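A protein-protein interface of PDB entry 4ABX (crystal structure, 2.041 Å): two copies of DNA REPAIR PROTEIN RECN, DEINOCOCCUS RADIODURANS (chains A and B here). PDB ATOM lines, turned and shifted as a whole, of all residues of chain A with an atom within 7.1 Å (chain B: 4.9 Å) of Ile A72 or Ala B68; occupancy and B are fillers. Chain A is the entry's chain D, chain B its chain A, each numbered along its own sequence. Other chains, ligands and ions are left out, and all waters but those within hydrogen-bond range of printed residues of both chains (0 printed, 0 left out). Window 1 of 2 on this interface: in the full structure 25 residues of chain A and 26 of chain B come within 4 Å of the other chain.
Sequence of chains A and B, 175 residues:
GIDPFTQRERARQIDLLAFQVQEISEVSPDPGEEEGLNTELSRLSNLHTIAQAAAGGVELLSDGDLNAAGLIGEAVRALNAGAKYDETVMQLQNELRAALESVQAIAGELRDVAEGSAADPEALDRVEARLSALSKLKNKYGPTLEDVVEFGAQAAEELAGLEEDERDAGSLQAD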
ATOM      1  N   LEU A  60     -19.859   4.221 -21.040  1.00  0.00           N
ATOM      2  CA  LEU A  60     -19.153   5.275 -20.313  1.00  0.00           C
ATOM      3  C   LEU A  60     -20.075   6.381 -19.792  1.00  0.00           C
ATOM      4  O   LEU A  60     -19.794   7.003 -18.763  1.00  0.00           O
ATOM      5  CB  LEU A  60     -18.065   5.881 -21.207  1.00  0.00           C
ATOM      6  CG  LEU A  60     -16.880   4.948 -21.480  1.00  0.00           C
ATOM      7  CD1 LEU A  60     -16.110   5.350 -22.734  1.00  0.00           C
ATOM      8  CD2 LEU A  60     -15.957   4.886 -20.266  1.00  0.00           C
ATOM      9  N   LEU A  61     -21.171   6.629 -20.498  1.00  0.00           N
ATOM     10  CA  LEU A  61     -22.058   7.734 -20.145  1.00  0.00           C
ATOM     11  C   LEU A  61     -23.158   7.332 -19.171  1.00  0.00           C
ATOM     12  O   LEU A  61     -23.609   8.153 -18.374  1.00  0.00           O
ATOM     13  CB  LEU A  61     -22.714   8.340 -21.390  1.00  0.00           C
ATOM     14  CG  LEU A  61     -21.874   9.092 -22.422  1.00  0.00           C
ATOM     15  CD1 LEU A  61     -22.781   9.666 -23.502  1.00  0.00           C
ATOM     16  CD2 LEU A  61     -21.033  10.196 -21.787  1.00  0.00           C
ATOM     17  N   ASN A  67     -19.969   5.499 -14.494  1.00  0.00           N
ATOM     18  CA  ASN A  67     -20.451   6.244 -15.651  1.00  0.00           C
ATOM     19  C   ASN A  67     -20.630   7.731 -15.385  1.00  0.00           C
ATOM     20  O   ASN A  67     -20.804   8.155 -14.238  1.00  0.00           O
ATOM     21  CB  ASN A  67     -21.752   5.638 -16.175  1.00  0.00           C
ATOM     22  CG  ASN A  67     -22.849   5.637 -15.135  1.00  0.00           C
ATOM     23  OD1 ASN A  67     -22.973   4.699 -14.343  1.00  0.00           O
ATOM     24  ND2 ASN A  67     -23.656   6.688 -15.132  1.00  0.00           N
ATOM     25  N   ALA A  68     -20.599   8.513 -16.461  1.00  0.00           N
ATOM     26  CA  ALA A  68     -20.622   9.969 -16.366  1.00  0.00           C
ATOM     27  C   ALA A  68     -21.891  10.507 -15.708  1.00  0.00           C
ATOM     28  O   ALA A  68     -21.819  11.343 -14.811  1.00  0.00           O
ATOM     29  CB  ALA A  68     -20.425  10.590 -17.740  1.00  0.00           C
ATOM     30  N   ALA A  69     -23.046  10.029 -16.158  1.00  0.00           N
ATOM     31  CA  ALA A  69     -24.324  10.472 -15.608  1.00  0.00           C
ATOM     32  C   ALA A  69     -24.371  10.232 -14.107  1.00  0.00           C
ATOM     33  O   ALA A  69     -24.930  11.031 -13.361  1.00  0.00           O
ATOM     34  CB  ALA A  69     -25.473   9.748 -16.284  1.00  0.00           C
ATOM     35  N   GLY A  70     -23.778   9.123 -13.678  1.00  0.00           N
ATOM     36  CA  GLY A  70     -23.736   8.758 -12.276  1.00  0.00           C
ATOM     37  C   GLY A  70     -22.949   9.749 -11.436  1.00  0.00           C
ATOM     38  O   GLY A  70     -23.377  10.114 -10.342  1.00  0.00           O
ATOM     39  N   LEU A  71     -21.801  10.188 -11.943  1.00  0.00           N
ATOM     40  CA  LEU A  71     -20.972  11.136 -11.203  1.00  0.00           C
ATOM     41  C   LEU A  71     -21.611  12.524 -11.181  1.00  0.00           C
ATOM     42  O   LEU A  71     -21.590  13.209 -10.158  1.00  0.00           O
ATOM     43  CB  LEU A  71     -19.555  11.195 -11.783  1.00  0.00           C
ATOM     44  CG  LEU A  71     -18.772   9.882 -11.690  1.00  0.00           C
ATOM     45  CD1 LEU A  71     -17.337  10.064 -12.170  1.00  0.00           C
ATOM     46  CD2 LEU A  71     -18.799   9.355 -10.266  1.00  0.00           C
ATOM     47  N   ILE A  72     -22.184  12.933 -12.310  1.00  0.00           N
ATOM     48  CA  ILE A  72     -22.855  14.230 -12.392  1.00  0.00           C
ATOM     49  C   ILE A  72     -24.028  14.292 -11.411  1.00  0.00           C
ATOM     50  O   ILE A  72     -24.232  15.304 -10.741  1.00  0.00           O
ATOM     51  CB  ILE A  72     -23.328  14.528 -13.827  1.00  0.00           C
ATOM     52  CG1 ILE A  72     -22.122  14.596 -14.769  1.00  0.00           C
ATOM     53  CG2 ILE A  72     -24.114  15.831 -13.882  1.00  0.00           C
ATOM     54  CD1 ILE A  72     -22.486  14.674 -16.232  1.00  0.00           C
ATOM     55  N   GLY A  73     -24.785  13.202 -11.323  1.00  0.00           N
ATOM     56  CA  GLY A  73     -25.863  13.086 -10.355  1.00  0.00           C
ATOM     57  C   GLY A  73     -25.381  13.217  -8.918  1.00  0.00           C
ATOM     58  O   GLY A  73     -26.037  13.859  -8.098  1.00  0.00           O
ATOM     59  N   GLU A  74     -24.241  12.606  -8.605  1.00  0.00           N
ATOM     60  CA  GLU A  74     -23.643  12.749  -7.275  1.00  0.00           C
ATOM     61  C   GLU A  74     -23.224  14.194  -7.001  1.00  0.00           C
ATOM     62  O   GLU A  74     -23.422  14.706  -5.901  1.00  0.00           O
ATOM     63  CB  GLU A  74     -22.441  11.815  -7.100  1.00  0.00           C
ATOM     64  CG  GLU A  74     -22.806  10.361  -6.887  1.00  0.00           C
ATOM     65  CD  GLU A  74     -21.588   9.454  -6.843  1.00  0.00           C
ATOM     66  OE1 GLU A  74     -20.632   9.770  -6.100  1.00  0.00           O
ATOM     67  OE2 GLU A  74     -21.591   8.433  -7.562  1.00  0.00           O
ATOM     68  N   ALA A  75     -22.632  14.835  -8.007  1.00  0.00           N
ATOM     69  CA  ALA A  75     -22.264  16.248  -7.929  1.00  0.00           C
ATOM     70  C   ALA A  75     -23.481  17.135  -7.652  1.00  0.00           C
ATOM     71  O   ALA A  75     -23.458  17.964  -6.745  1.00  0.00           O
ATOM     72  CB  ALA A  75     -21.570  16.684  -9.219  1.00  0.00           C
ATOM     73  N   VAL A  76     -24.540  16.955  -8.437  1.00  0.00           N
ATOM     74  CA  VAL A  76     -25.804  17.664  -8.215  1.00  0.00           C
ATOM     75  C   VAL A  76     -26.282  17.547  -6.768  1.00  0.00           C
ATOM     76  O   VAL A  76     -26.693  18.537  -6.161  1.00  0.00           O
ATOM     77  CB  VAL A  76     -26.918  17.132  -9.148  1.00  0.00           C
ATOM     78  CG1 VAL A  76     -28.290  17.633  -8.698  1.00  0.00           C
ATOM     79  CG2 VAL A  76     -26.647  17.540 -10.582  1.00  0.00           C
ATOM     80  N   ARG A  77     -26.230  16.332  -6.219  1.00  0.00           N
ATOM     81  CA  ARG A  77     -26.673  16.090  -4.852  1.00  0.00           C
ATOM     82  C   ARG A  77     -25.759  16.741  -3.811  1.00  0.00           C
ATOM     83  O   ARG A  77     -26.220  17.203  -2.770  1.00  0.00           O
ATOM     84  CB  ARG A  77     -26.811  14.588  -4.572  1.00  0.00           C
ATOM     85  CG  ARG A  77     -28.081  13.962  -5.148  1.00  0.00           C
ATOM     86  CD  ARG A  77     -28.296  12.529  -4.655  1.00  0.00           C
ATOM     87  NE  ARG A  77     -27.315  11.599  -5.208  1.00  0.00           N
ATOM     88  CZ  ARG A  77     -27.372  11.095  -6.440  1.00  0.00           C
ATOM     89  NH1 ARG A  77     -28.360  11.439  -7.256  1.00  0.00           N
ATOM     90  NH2 ARG A  77     -26.439  10.251  -6.860  1.00  0.00           N
ATOM     91  N   ALA A  78     -24.464  16.764  -4.092  1.00  0.00           N
ATOM     92  CA  ALA A  78     -23.505  17.379  -3.183  1.00  0.00           C
ATOM     93  C   ALA A  78     -23.672  18.901  -3.134  1.00  0.00           C
ATOM     94  O   ALA A  78     -23.213  19.558  -2.198  1.00  0.00           O
ATOM     95  CB  ALA A  78     -22.085  17.005  -3.585  1.00  0.00           C
ATOM     96  N   LEU A  96     -26.044  22.311 -13.908  1.00  0.00           N
ATOM     97  CA  LEU A  96     -25.521  20.947 -13.858  1.00  0.00           C
ATOM     98  C   LEU A  96     -26.625  19.914 -14.124  1.00  0.00           C
ATOM     99  O   LEU A  96     -26.380  18.889 -14.756  1.00  0.00           O
ATOM    100  CB  LEU A  96     -24.825  20.686 -12.522  1.00  0.00           C
ATOM    101  CG  LEU A  96     -23.904  19.469 -12.456  1.00  0.00           C
ATOM    102  CD1 LEU A  96     -22.815  19.575 -13.517  1.00  0.00           C
ATOM    103  CD2 LEU A  96     -23.295  19.330 -11.062  1.00  0.00           C
ATOM    104  N   ARG A  97     -27.839  20.186 -13.647  1.00  0.00           N
ATOM    105  CA  ARG A  97     -28.982  19.327 -13.949  1.00  0.00           C
ATOM    106  C   ARG A  97     -29.234  19.297 -15.455  1.00  0.00           C
ATOM    107  O   ARG A  97     -29.554  18.252 -16.012  1.00  0.00           O
ATOM    108  CB  ARG A  97     -30.252  19.819 -13.250  1.00  0.00           C
ATOM    109  CG  ARG A  97     -30.249  19.736 -11.732  1.00  0.00           C
ATOM    110  CD  ARG A  97     -31.653  20.009 -11.205  1.00  0.00           C
ATOM    111  NE  ARG A  97     -31.690  20.279  -9.771  1.00  0.00           N
ATOM    112  CZ  ARG A  97     -31.751  19.335  -8.837  1.00  0.00           C
ATOM    113  NH1 ARG A  97     -31.769  18.054  -9.186  1.00  0.00           N
ATOM    114  NH2 ARG A  97     -31.787  19.672  -7.552  1.00  0.00           N
ATOM    115  N   ALA A  99     -26.979  19.885 -17.828  1.00  0.00           N
ATOM    116  CA  ALA A  99     -25.881  19.091 -18.377  1.00  0.00           C
ATOM    117  C   ALA A  99     -26.168  17.591 -18.233  1.00  0.00           C
ATOM    118  O   ALA A  99     -25.929  16.810 -19.155  1.00  0.00           O
ATOM    119  CB  ALA A  99     -24.567  19.446 -17.687  1.00  0.00           C
ATOM    120  N   LEU A 100     -26.679  17.200 -17.068  1.00  0.00           N
ATOM    121  CA  LEU A 100     -27.055  15.812 -16.813  1.00  0.00           C
ATOM    122  C   LEU A 100     -28.085  15.332 -17.833  1.00  0.00           C
ATOM    123  O   LEU A 100     -27.913  14.288 -18.454  1.00  0.00           O
ATOM    124  CB  LEU A 100     -27.612  15.651 -15.392  1.00  0.00           C
ATOM    125  CG  LEU A 100     -28.042  14.226 -15.019  1.00  0.00           C
ATOM    126  CD1 LEU A 100     -26.925  13.234 -15.339  1.00  0.00           C
ATOM    127  CD2 LEU A 100     -28.443  14.138 -13.548  1.00  0.00           C
ATOM    128  N   GLU A 101     -29.157  16.101 -17.994  1.00  0.00           N
ATOM    129  CA  GLU A 101     -30.203  15.775 -18.960  1.00  0.00           C
ATOM    130  C   GLU A 101     -29.670  15.635 -20.383  1.00  0.00           C
ATOM    131  O   GLU A 101     -30.144  14.799 -21.148  1.00  0.00           O
ATOM    132  CB  GLU A 101     -31.317  16.824 -18.922  1.00  0.00           C
ATOM    133  CG  GLU A 101     -32.169  16.750 -17.663  1.00  0.00           C
ATOM    134  CD  GLU A 101     -33.125  17.923 -17.517  1.00  0.00           C
ATOM    135  OE1 GLU A 101     -33.375  18.628 -18.521  1.00  0.00           O
ATOM    136  OE2 GLU A 101     -33.624  18.137 -16.391  1.00  0.00           O
ATOM    137  N   VAL A 103     -26.532  14.744 -21.223  1.00  0.00           N
ATOM    138  CA  VAL A 103     -25.735  13.520 -21.264  1.00  0.00           C
ATOM    139  C   VAL A 103     -26.645  12.304 -21.377  1.00  0.00           C
ATOM    140  O   VAL A 103     -26.365  11.396 -22.141  1.00  0.00           O
ATOM    141  CB  VAL A 103     -24.805  13.392 -20.034  1.00  0.00           C
ATOM    142  CG1 VAL A 103     -24.213  12.000 -19.950  1.00  0.00           C
ATOM    143  CG2 VAL A 103     -23.693  14.431 -20.108  1.00  0.00           C
ATOM    144  N   LEU B  60     -15.903  15.781  -7.786  1.00  0.00           N
ATOM    145  CA  LEU B  60     -16.669  14.807  -8.565  1.00  0.00           C
ATOM    146  C   LEU B  60     -16.746  15.146 -10.050  1.00  0.00           C
ATOM    147  O   LEU B  60     -16.845  14.254 -10.897  1.00  0.00           O
ATOM    148  CB  LEU B  60     -18.089  14.669  -8.006  1.00  0.00           C
ATOM    149  CG  LEU B  60     -18.257  14.016  -6.632  1.00  0.00           C
ATOM    150  CD1 LEU B  60     -19.609  14.383  -6.018  1.00  0.00           C
ATOM    151  CD2 LEU B  60     -18.080  12.503  -6.698  1.00  0.00           C
ATOM    152  N   LEU B  61     -16.715  16.434 -10.372  1.00  0.00           N
ATOM    153  CA  LEU B  61     -16.841  16.846 -11.762  1.00  0.00           C
ATOM    154  C   LEU B  61     -15.496  16.840 -12.482  1.00  0.00           C
ATOM    155  O   LEU B  61     -15.445  16.657 -13.695  1.00  0.00           O
ATOM    156  CB  LEU B  61     -17.470  18.239 -11.874  1.00  0.00           C
ATOM    157  CG  LEU B  61     -18.948  18.410 -11.514  1.00  0.00           C
ATOM    158  CD1 LEU B  61     -19.388  19.830 -11.825  1.00  0.00           C
ATOM    159  CD2 LEU B  61     -19.824  17.395 -12.258  1.00  0.00           C
ATOM    160  N   SER B  62     -14.410  17.023 -11.734  1.00  0.00           N
ATOM    161  CA  SER B  62     -13.146  17.389 -12.362  1.00  0.00           C
ATOM    162  C   SER B  62     -11.869  16.845 -11.706  1.00  0.00           C
ATOM    163  O   SER B  62     -11.043  16.234 -12.378  1.00  0.00           O
ATOM    164  CB  SER B  62     -13.060  18.917 -12.473  1.00  0.00           C
ATOM    165  OG  SER B  62     -11.933  19.316 -13.234  1.00  0.00           O
ATOM    166  N   LEU B  66     -11.380   9.661 -10.128  1.00  0.00           N
ATOM    167  CA  LEU B  66     -12.525   9.376 -10.979  1.00  0.00           C
ATOM    168  C   LEU B  66     -13.426  10.609 -11.008  1.00  0.00           C
ATOM    169  O   LEU B  66     -13.939  11.039  -9.969  1.00  0.00           O
ATOM    170  CB  LEU B  66     -13.306   8.172 -10.451  1.00  0.00           C
ATOM    171  CG  LEU B  66     -14.439   7.687 -11.361  1.00  0.00           C
ATOM    172  CD1 LEU B  66     -13.878   7.056 -12.626  1.00  0.00           C
ATOM    173  CD2 LEU B  66     -15.342   6.705 -10.632  1.00  0.00           C
ATOM    174  N   ASN B  67     -13.610  11.185 -12.189  1.00  0.00           N
ATOM    175  CA  ASN B  67     -14.422  12.391 -12.312  1.00  0.00           C
ATOM    176  C   ASN B  67     -15.293  12.410 -13.562  1.00  0.00           C
ATOM    177  O   ASN B  67     -15.023  11.707 -14.540  1.00  0.00           O
ATOM    178  CB  ASN B  67     -13.541  13.643 -12.245  1.00  0.00           C
ATOM    179  CG  ASN B  67     -12.594  13.756 -13.424  1.00  0.00           C
ATOM    180  OD1 ASN B  67     -12.963  14.255 -14.487  1.00  0.00           O
ATOM    181  ND2 ASN B  67     -11.363  13.295 -13.241  1.00  0.00           N
ATOM    182  N   ALA B  68     -16.342  13.222 -13.520  1.00  0.00           N
ATOM    183  CA  ALA B  68     -17.305  13.297 -14.607  1.00  0.00           C
ATOM    184  C   ALA B  68     -16.677  13.725 -15.939  1.00  0.00           C
ATOM    185  O   ALA B  68     -16.914  13.095 -16.972  1.00  0.00           O
ATOM    186  CB  ALA B  68     -18.448  14.227 -14.229  1.00  0.00           C
ATOM    187  N   ALA B  69     -15.878  14.789 -15.915  1.00  0.00           N
ATOM    188  CA  ALA B  69     -15.263  15.302 -17.137  1.00  0.00           C
ATOM    189  C   ALA B  69     -14.384  14.243 -17.802  1.00  0.00           C
ATOM    190  O   ALA B  69     -14.386  14.097 -19.023  1.00  0.00           O
ATOM    191  CB  ALA B  69     -14.451  16.562 -16.845  1.00  0.00           C
ATOM    192  N   GLY B  70     -13.633  13.510 -16.986  1.00  0.00           N
ATOM    193  CA  GLY B  70     -12.780  12.443 -17.480  1.00  0.00           C
ATOM    194  C   GLY B  70     -13.560  11.358 -18.196  1.00  0.00           C
ATOM    195  O   GLY B  70     -13.147  10.879 -19.249  1.00  0.00           O
ATOM    196  N   LEU B  71     -14.698  10.965 -17.632  1.00  0.00           N
ATOM    197  CA  LEU B  71     -15.516   9.931 -18.264  1.00  0.00           C
ATOM    198  C   LEU B  71     -16.165  10.416 -19.554  1.00  0.00           C
ATOM    199  O   LEU B  71     -16.239   9.679 -20.539  1.00  0.00           O
ATOM    200  CB  LEU B  71     -16.572   9.394 -17.297  1.00  0.00           C
ATOM    201  CG  LEU B  71     -15.960   8.662 -16.105  1.00  0.00           C
ATOM    202  CD1 LEU B  71     -17.049   8.124 -15.194  1.00  0.00           C
ATOM    203  CD2 LEU B  71     -15.052   7.540 -16.589  1.00  0.00           C
ATOM    204  N   ILE B  72     -16.636  11.656 -19.550  1.00  0.00           N
ATOM    205  CA  ILE B  72     -17.206  12.240 -20.754  1.00  0.00           C
ATOM    206  C   ILE B  72     -16.156  12.251 -21.866  1.00  0.00           C
ATOM    207  O   ILE B  72     -16.451  11.939 -23.018  1.00  0.00           O
ATOM    208  CB  ILE B  72     -17.746  13.666 -20.494  1.00  0.00           C
ATOM    209  CG1 ILE B  72     -18.879  13.624 -19.461  1.00  0.00           C
ATOM    210  CG2 ILE B  72     -18.231  14.311 -21.791  1.00  0.00           C
ATOM    211  CD1 ILE B  72     -19.492  14.995 -19.154  1.00  0.00           C
ATOM    212  N   VAL B 103     -19.677  21.171 -18.290  1.00  0.00           N
ATOM    213  CA  VAL B 103     -19.299  20.552 -17.025  1.00  0.00           C
ATOM    214  C   VAL B 103     -18.004  21.149 -16.483  1.00  0.00           C
ATOM    215  O   VAL B 103     -17.886  21.402 -15.285  1.00  0.00           O
ATOM    216  CB  VAL B 103     -19.180  19.012 -17.148  1.00  0.00           C
ATOM    217  CG1 VAL B 103     -18.393  18.443 -15.984  1.00  0.00           C
ATOM    218  CG2 VAL B 103     -20.567  18.381 -17.214  1.00  0.00           C
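The backbone NH of Ala B68 sits at hydrogen-bond distance from the backbone carbonyl oxygen of Leu B60.
The backbone carbonyl oxygen of Leu A60 sits at hydrogen-bond distance from the backbone NH of Ala A68, at 2.9 Å.
The backbone NH (N) of Gly A70 sits close to the side-chain amide nitrogen (ND2) of Asn A67 (2.8 Å).
The backbone carbonyl oxygen of Leu B61 is in hydrogen-bond range of the backbone NH of Ala B69, at 2.9 Å.
ND2 of Asn B67 is in hydrogen-bond range of O of Ser B62 (3.1 Å).
The side-chain amide oxygen of Asn B67 sits at hydrogen-bond distance from the backbone NH of Ala B69 (3.3 Å).
Asn A67 touches Leu B71, and with the chains exchanged Leu A71 touches Asn B67.
Ala A68 touches Leu B71, and with the chains exchanged Leu A71 touches Ala B68.
Ala A68 touches Ile B72, and with the chains exchanged Ile A72 touches Ala B68.
Leu A71 touches its own counterpart, Leu B71.
Of the 12 pairs that touch across the chains among the printed residues, 7 have their exchanged pair printed and touching as well.
Leu B71 touches Asn A67.
Leu B71 touches Ala A68.
Ala A68 touches Ile B72.
C of Asn B67 touches CD1 of Leu A71, at 3.4 Å.
Ala B68 touches Leu A71.
Leu A71 touches Leu B71 (CD1 to CD1, 3.6 Å).
Ala B68 touches Ile A72 (CB to CG1, 3.7 Å).
Ala A75 touches Leu B60 (N to CD1, 3.6 Å).
Ala A75 touches Leu B61.
CD1 of Leu B61 touches CD1 of Leu A96 (3.8 Å).
Hydrophobic or aromatic side chains of chain A that line the printed part of chain B: Ala A68, Leu A71, Ile A72, Ala A75 and Leu A96.
Hydrophobic or aromatic side chains of chain B within 4 Å of the printed part of chain A: Leu B60, Leu B61, Leu B66, Ala B68, Leu B71 and Ile B72.
Along chain B the printed residues that touch a printed residue of chain A span positions 60 to 72.
Among the printed residues, 12 pairs touch across the chains.
Gly A73 touches none of the printed residues of chain B.
Printed residues of chain B within 4 Å of Glu A74: Leu B60 (3.8 Å).
Of the printed residues of chain A, Leu B60 touches Glu A74 (3.8 Å) and Ala A75 (3.6 Å).
Of chain A, only Leu A71 and Ile A72 come within 4 Å of Ala B68.
Ala B69 touches none of the printed residues of chain A.
The nearest residue of chain A that does not touch Ala B68 is Ala A68 (4.4 Å).
The nearest printed residue of chain A that does not touch Ile B72 is Ile A72 (4.2 Å).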
